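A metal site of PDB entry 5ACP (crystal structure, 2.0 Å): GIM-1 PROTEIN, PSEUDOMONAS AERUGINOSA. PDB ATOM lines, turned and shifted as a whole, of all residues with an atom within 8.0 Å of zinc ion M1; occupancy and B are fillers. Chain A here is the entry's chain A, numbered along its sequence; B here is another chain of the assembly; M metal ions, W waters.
OD2 of OCS 175 touches zinc ion M1 (3.5 Å). Four residues have an atom within 4 Å of zinc ion M1: His 94, His 96, His 156 and OCS 175.
Zinc ion M1 is bound by water W1, at 1.9 Å. Zinc ion M1 is bound by a ring nitrogen (NE2) of His 156, 2.0 Å away. A ring nitrogen (ND1) of His 96 binds zinc ion M1 (2.1 Å). NE2 of His 94 binds zinc ion M1.
The backbone NH of His 156 lies within hydrogen-bond range of the side-chain amide oxygen of Asn 160 (3.0 Å). NE2 of His 96 sits at hydrogen-bond distance from OD2 of Asp 190, at 2.7 Å. OD3 of OCS 175 lies within salt-bridge range of the guanidinium group (NE) of Arg 99 (2.8 Å).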
ATOM      1  N   THR A  93      -2.140  22.876 -25.078  1.00  0.00           N
ATOM      2  CA  THR A  93      -1.437  21.606 -24.908  1.00  0.00           C
ATOM      3  C   THR A  93      -2.343  20.375 -24.900  1.00  0.00           C
ATOM      4  O   THR A  93      -1.852  19.247 -24.850  1.00  0.00           O
ATOM      5  CB  THR A  93      -0.598  21.633 -23.598  1.00  0.00           C
ATOM      6  OG1 THR A  93      -1.437  21.917 -22.480  1.00  0.00           O
ATOM      7  CG2 THR A  93       0.502  22.690 -23.684  1.00  0.00           C
ATOM      8  N   HIS A  94      -3.661  20.581 -24.926  1.00  0.00           N
ATOM      9  CA  HIS A  94      -4.619  19.565 -25.362  1.00  0.00           C
ATOM     10  C   HIS A  94      -5.977  20.241 -25.477  1.00  0.00           C
ATOM     11  O   HIS A  94      -6.066  21.452 -25.353  1.00  0.00           O
ATOM     12  CB  HIS A  94      -4.678  18.347 -24.423  1.00  0.00           C
ATOM     13  CG  HIS A  94      -5.149  18.633 -23.034  1.00  0.00           C
ATOM     14  ND1 HIS A  94      -4.330  19.147 -22.065  1.00  0.00           N
ATOM     15  CD2 HIS A  94      -6.351  18.403 -22.445  1.00  0.00           C
ATOM     16  CE1 HIS A  94      -5.016  19.257 -20.930  1.00  0.00           C
ATOM     17  NE2 HIS A  94      -6.237  18.820 -21.134  1.00  0.00           N
ATOM     18  N   SER A  95      -7.029  19.470 -25.738  1.00  0.00           N
ATOM     19  CA  SER A  95      -8.280  20.065 -26.205  1.00  0.00           C
ATOM     20  C   SER A  95      -9.203  20.559 -25.095  1.00  0.00           C
ATOM     21  O   SER A  95     -10.168  21.274 -25.368  1.00  0.00           O
ATOM     22  CB  SER A  95      -9.040  19.080 -27.092  1.00  0.00           C
ATOM     23  OG  SER A  95      -9.655  18.048 -26.330  1.00  0.00           O
ATOM     24  N   HIS A  96      -8.920  20.189 -23.848  1.00  0.00           N
ATOM     25  CA  HIS A  96      -9.838  20.498 -22.750  1.00  0.00           C
ATOM     26  C   HIS A  96      -9.992  22.003 -22.506  1.00  0.00           C
ATOM     27  O   HIS A  96      -9.083  22.796 -22.758  1.00  0.00           O
ATOM     28  CB  HIS A  96      -9.374  19.819 -21.470  1.00  0.00           C
ATOM     29  CG  HIS A  96      -9.685  18.359 -21.410  1.00  0.00           C
ATOM     30  ND1 HIS A  96      -9.200  17.543 -20.413  1.00  0.00           N
ATOM     31  CD2 HIS A  96     -10.435  17.570 -22.214  1.00  0.00           C
ATOM     32  CE1 HIS A  96      -9.637  16.301 -20.612  1.00  0.00           C
ATOM     33  NE2 HIS A  96     -10.386  16.299 -21.694  1.00  0.00           N
ATOM     34  N   GLU A  97     -11.169  22.356 -21.992  1.00  0.00           N
ATOM     35  CA  GLU A  97     -11.582  23.746 -21.737  1.00  0.00           C
ATOM     36  C   GLU A  97     -10.518  24.608 -21.051  1.00  0.00           C
ATOM     37  O   GLU A  97     -10.348  25.782 -21.408  1.00  0.00           O
ATOM     38  CB  GLU A  97     -12.847  23.734 -20.880  1.00  0.00           C
ATOM     39  CG  GLU A  97     -13.541  25.076 -20.760  1.00  0.00           C
ATOM     40  CD  GLU A  97     -14.263  25.483 -22.028  1.00  0.00           C
ATOM     41  OE1 GLU A  97     -14.300  24.681 -22.975  1.00  0.00           O
ATOM     42  OE2 GLU A  97     -14.813  26.606 -22.063  1.00  0.00           O
ATOM     43  N   ASP A  98      -9.831  24.044 -20.071  1.00  0.00           N
ATOM     44  CA  ASP A  98      -8.865  24.817 -19.284  1.00  0.00           C
ATOM     45  C   ASP A  98      -7.611  25.149 -20.082  1.00  0.00           C
ATOM     46  O   ASP A  98      -6.784  25.948 -19.645  1.00  0.00           O
ATOM     47  CB  ASP A  98      -8.502  24.072 -18.006  1.00  0.00           C
ATOM     48  CG  ASP A  98      -7.900  22.711 -18.269  1.00  0.00           C
ATOM     49  OD1 ASP A  98      -8.587  21.841 -18.842  1.00  0.00           O
ATOM     50  OD2 ASP A  98      -6.732  22.499 -17.875  1.00  0.00           O
ATOM     51  N   ARG A  99      -7.480  24.531 -21.255  1.00  0.00           N
ATOM     52  CA  ARG A  99      -6.363  24.795 -22.161  1.00  0.00           C
ATOM     53  C   ARG A  99      -6.761  25.676 -23.349  1.00  0.00           C
ATOM     54  O   ARG A  99      -5.906  26.333 -23.954  1.00  0.00           O
ATOM     55  CB  ARG A  99      -5.786  23.481 -22.695  1.00  0.00           C
ATOM     56  CG  ARG A  99      -5.476  22.430 -21.635  1.00  0.00           C
ATOM     57  CD  ARG A  99      -4.339  22.865 -20.744  1.00  0.00           C
ATOM     58  NE  ARG A  99      -4.742  23.072 -19.358  1.00  0.00           N
ATOM     59  CZ  ARG A  99      -4.035  23.781 -18.477  1.00  0.00           C
ATOM     60  NH1 ARG A  99      -2.904  24.377 -18.849  1.00  0.00           N
ATOM     61  NH2 ARG A  99      -4.457  23.916 -17.224  1.00  0.00           N
ATOM     62  N   HIS A 156      -2.925  11.851 -19.633  1.00  0.00           N
ATOM     63  CA  HIS A 156      -4.116  12.561 -19.168  1.00  0.00           C
ATOM     64  C   HIS A 156      -5.177  12.553 -20.261  1.00  0.00           C
ATOM     65  O   HIS A 156      -6.377  12.396 -19.995  1.00  0.00           O
ATOM     66  CB  HIS A 156      -3.765  13.986 -18.759  1.00  0.00           C
ATOM     67  CG  HIS A 156      -4.945  14.870 -18.546  1.00  0.00           C
ATOM     68  ND1 HIS A 156      -5.738  14.815 -17.414  1.00  0.00           N
ATOM     69  CD2 HIS A 156      -5.477  15.862 -19.312  1.00  0.00           C
ATOM     70  CE1 HIS A 156      -6.690  15.712 -17.496  1.00  0.00           C
ATOM     71  NE2 HIS A 156      -6.562  16.363 -18.647  1.00  0.00           N
ATOM     72  N   THR A 157      -4.717  12.748 -21.499  1.00  0.00           N
ATOM     73  CA  THR A 157      -5.556  12.604 -22.694  1.00  0.00           C
ATOM     74  C   THR A 157      -4.775  11.959 -23.848  1.00  0.00           C
ATOM     75  O   THR A 157      -3.558  11.801 -23.755  1.00  0.00           O
ATOM     76  CB  THR A 157      -6.079  13.955 -23.191  1.00  0.00           C
ATOM     77  OG1 THR A 157      -4.981  14.866 -23.349  1.00  0.00           O
ATOM     78  CG2 THR A 157      -7.094  14.539 -22.216  1.00  0.00           C
ATOM     79  N   ASP A 159      -4.131  13.332 -26.581  1.00  0.00           N
ATOM     80  CA  ASP A 159      -3.495  14.362 -27.374  1.00  0.00           C
ATOM     81  C   ASP A 159      -2.536  15.278 -26.605  1.00  0.00           C
ATOM     82  O   ASP A 159      -1.996  16.218 -27.193  1.00  0.00           O
ATOM     83  CB  ASP A 159      -4.572  15.227 -28.036  1.00  0.00           C
ATOM     84  CG  ASP A 159      -5.450  15.944 -27.026  1.00  0.00           C
ATOM     85  OD1 ASP A 159      -5.838  15.324 -26.023  1.00  0.00           O
ATOM     86  OD2 ASP A 159      -5.752  17.140 -27.250  1.00  0.00           O
ATOM     87  N   ASN A 160      -2.335  15.040 -25.314  1.00  0.00           N
ATOM     88  CA  ASN A 160      -1.568  15.998 -24.524  1.00  0.00           C
ATOM     89  C   ASN A 160      -0.138  16.125 -25.014  1.00  0.00           C
ATOM     90  O   ASN A 160       0.537  15.136 -25.322  1.00  0.00           O
ATOM     91  CB  ASN A 160      -1.586  15.681 -23.019  1.00  0.00           C
ATOM     92  CG  ASN A 160      -1.307  14.220 -22.688  1.00  0.00           C
ATOM     93  OD1 ASN A 160      -1.909  13.659 -21.764  1.00  0.00           O
ATOM     94  ND2 ASN A 160      -0.382  13.596 -23.423  1.00  0.00           N
ATOM     95  N   GLY A 174       1.758  20.713 -18.356  1.00  0.00           N
ATOM     96  CA  GLY A 174       0.308  20.719 -18.419  1.00  0.00           C
ATOM     97  C   GLY A 174      -0.297  19.651 -17.528  1.00  0.00           C
ATOM     98  O   GLY A 174       0.234  19.341 -16.466  1.00  0.00           O
ATOM     99  N   OCS A 175      -1.416  19.070 -17.964  1.00  0.00           N
ATOM    100  CA  OCS A 175      -2.134  18.090 -17.144  1.00  0.00           C
ATOM    101  CB  OCS A 175      -3.621  18.133 -17.479  1.00  0.00           C
ATOM    102  SG  OCS A 175      -4.322  19.737 -17.087  1.00  0.00           S
ATOM    103  C   OCS A 175      -1.602  16.680 -17.260  1.00  0.00           C
ATOM    104  O   OCS A 175      -2.084  15.763 -16.597  1.00  0.00           O
ATOM    105  OD1 OCS A 175      -3.689  20.201 -15.912  1.00  0.00           O
ATOM    106  OD2 OCS A 175      -5.719  19.634 -16.849  1.00  0.00           O
ATOM    107  OD3 OCS A 175      -4.047  20.647 -18.141  1.00  0.00           O
ATOM    108  N   LEU A 176      -0.584  16.500 -18.091  1.00  0.00           N
ATOM    109  CA  LEU A 176       0.130  15.235 -18.167  1.00  0.00           C
ATOM    110  C   LEU A 176       0.930  15.007 -16.890  1.00  0.00           C
ATOM    111  O   LEU A 176       1.243  13.859 -16.552  1.00  0.00           O
ATOM    112  CB  LEU A 176       1.047  15.225 -19.391  1.00  0.00           C
ATOM    113  CG  LEU A 176       1.840  13.953 -19.669  1.00  0.00           C
ATOM    114  CD1 LEU A 176       0.945  12.726 -19.754  1.00  0.00           C
ATOM    115  CD2 LEU A 176       2.658  14.118 -20.939  1.00  0.00           C
ATOM    116  N   TYR A 187      -8.926  14.031 -13.188  1.00  0.00           N
ATOM    117  CA  TYR A 187      -9.908  13.597 -14.183  1.00  0.00           C
ATOM    118  C   TYR A 187      -9.301  12.587 -15.154  1.00  0.00           C
ATOM    119  O   TYR A 187      -8.444  12.936 -15.972  1.00  0.00           O
ATOM    120  CB  TYR A 187     -10.444  14.799 -14.971  1.00  0.00           C
ATOM    121  CG  TYR A 187     -11.490  14.431 -15.983  1.00  0.00           C
ATOM    122  CD1 TYR A 187     -12.793  14.150 -15.585  1.00  0.00           C
ATOM    123  CD2 TYR A 187     -11.190  14.362 -17.327  1.00  0.00           C
ATOM    124  CE1 TYR A 187     -13.765  13.816 -16.510  1.00  0.00           C
ATOM    125  CE2 TYR A 187     -12.146  14.032 -18.266  1.00  0.00           C
ATOM    126  CZ  TYR A 187     -13.432  13.750 -17.851  1.00  0.00           C
ATOM    127  OH  TYR A 187     -14.394  13.416 -18.779  1.00  0.00           O
ATOM    128  N   ASP A 190     -10.975  10.956 -19.876  1.00  0.00           N
ATOM    129  CA  ASP A 190     -10.396  10.939 -21.222  1.00  0.00           C
ATOM    130  C   ASP A 190      -8.987  10.359 -21.225  1.00  0.00           C
ATOM    131  O   ASP A 190      -8.253  10.494 -22.206  1.00  0.00           O
ATOM    132  CB  ASP A 190     -10.382  12.356 -21.803  1.00  0.00           C
ATOM    133  CG  ASP A 190     -11.766  12.908 -22.030  1.00  0.00           C
ATOM    134  OD1 ASP A 190     -12.636  12.159 -22.510  1.00  0.00           O
ATOM    135  OD2 ASP A 190     -11.994  14.102 -21.722  1.00  0.00           O
ATOM    136  N   HIS A 217      -2.326  22.325 -13.166  1.00  0.00           N
ATOM    137  CA  HIS A 217      -2.949  22.746 -11.906  1.00  0.00           C
ATOM    138  C   HIS A 217      -1.992  22.505 -10.755  1.00  0.00           C
ATOM    139  O   HIS A 217      -1.253  21.523 -10.754  1.00  0.00           O
ATOM    140  CB  HIS A 217      -4.261  22.024 -11.669  1.00  0.00           C
ATOM    141  CG  HIS A 217      -5.156  21.991 -12.861  1.00  0.00           C
ATOM    142  ND1 HIS A 217      -5.938  23.074 -13.227  1.00  0.00           N
ATOM    143  CD2 HIS A 217      -5.375  21.038 -13.781  1.00  0.00           C
ATOM    144  CE1 HIS A 217      -6.599  22.775 -14.333  1.00  0.00           C
ATOM    145  NE2 HIS A 217      -6.285  21.540 -14.689  1.00  0.00           N
ATOM    146  N   ILE B  42     -16.455  18.506 -14.739  1.00  0.00           N
ATOM    147  CA  ILE B  42     -15.813  19.819 -14.730  1.00  0.00           C
ATOM    148  C   ILE B  42     -14.456  19.702 -15.414  1.00  0.00           C
ATOM    149  O   ILE B  42     -13.488  19.231 -14.810  1.00  0.00           O
ATOM    150  CB  ILE B  42     -15.641  20.363 -13.305  1.00  0.00           C
ATOM    151  CG1 ILE B  42     -17.008  20.516 -12.623  1.00  0.00           C
ATOM    152  CG2 ILE B  42     -14.913  21.707 -13.330  1.00  0.00           C
ATOM    153  N   GLU B  43     -14.397  20.134 -16.665  1.00  0.00           N
ATOM    154  CA  GLU B  43     -13.168  20.033 -17.451  1.00  0.00           C
ATOM    155  C   GLU B  43     -12.052  20.841 -16.820  1.00  0.00           C
ATOM    156  O   GLU B  43     -12.135  22.069 -16.714  1.00  0.00           O
ATOM    157  CB  GLU B  43     -13.404  20.510 -18.891  1.00  0.00           C
ATOM    158  CG  GLU B  43     -14.450  19.703 -19.660  1.00  0.00           C
ATOM    159  CD  GLU B  43     -13.948  18.337 -20.092  1.00  0.00           C
ATOM    160  OE1 GLU B  43     -12.861  17.918 -19.614  1.00  0.00           O
ATOM    161  OE2 GLU B  43     -14.629  17.682 -20.907  1.00  0.00           O
ATOM    162  N   GLY B  44     -11.006  20.145 -16.376  1.00  0.00           N
ATOM    163  CA  GLY B  44      -9.842  20.783 -15.787  1.00  0.00           C
ATOM    164  C   GLY B  44      -9.662  20.462 -14.322  1.00  0.00           C
ATOM    165  O   GLY B  44      -8.857  21.092 -13.638  1.00  0.00           O
ATOM    166  N   TYR B  45     -10.407  19.496 -13.801  1.00  0.00           N
ATOM    167  CA  TYR B  45     -10.260  19.130 -12.394  1.00  0.00           C
ATOM    168  C   TYR B  45     -10.805  17.728 -12.071  1.00  0.00           C
ATOM    169  O   TYR B  45     -10.134  16.959 -11.375  1.00  0.00           O
ATOM    170  CB  TYR B  45     -10.959  20.177 -11.516  1.00  0.00           C
ATOM    171  CG  TYR B  45     -11.830  19.587 -10.443  1.00  0.00           C
ATOM    172  CD1 TYR B  45     -11.325  19.295  -9.179  1.00  0.00           C
ATOM    173  CD2 TYR B  45     -13.169  19.325 -10.686  1.00  0.00           C
ATOM    174  CE1 TYR B  45     -12.128  18.751  -8.196  1.00  0.00           C
ATOM    175  CE2 TYR B  45     -13.975  18.786  -9.712  1.00  0.00           C
ATOM    176  CZ  TYR B  45     -13.454  18.510  -8.467  1.00  0.00           C
ATOM    177  OH  TYR B  45     -14.259  17.971  -7.493  1.00  0.00           O
HETATM  178 ZN    ZN M   1      -7.466  18.004 -19.392  1.00  0.00          ZN
HETATM  179 ZN    ZN M   2      -6.635  21.120 -16.694  1.00  0.00          ZN
HETATM  180  O   HOH W   1      -7.676  19.444 -18.177  1.00  0.00           O
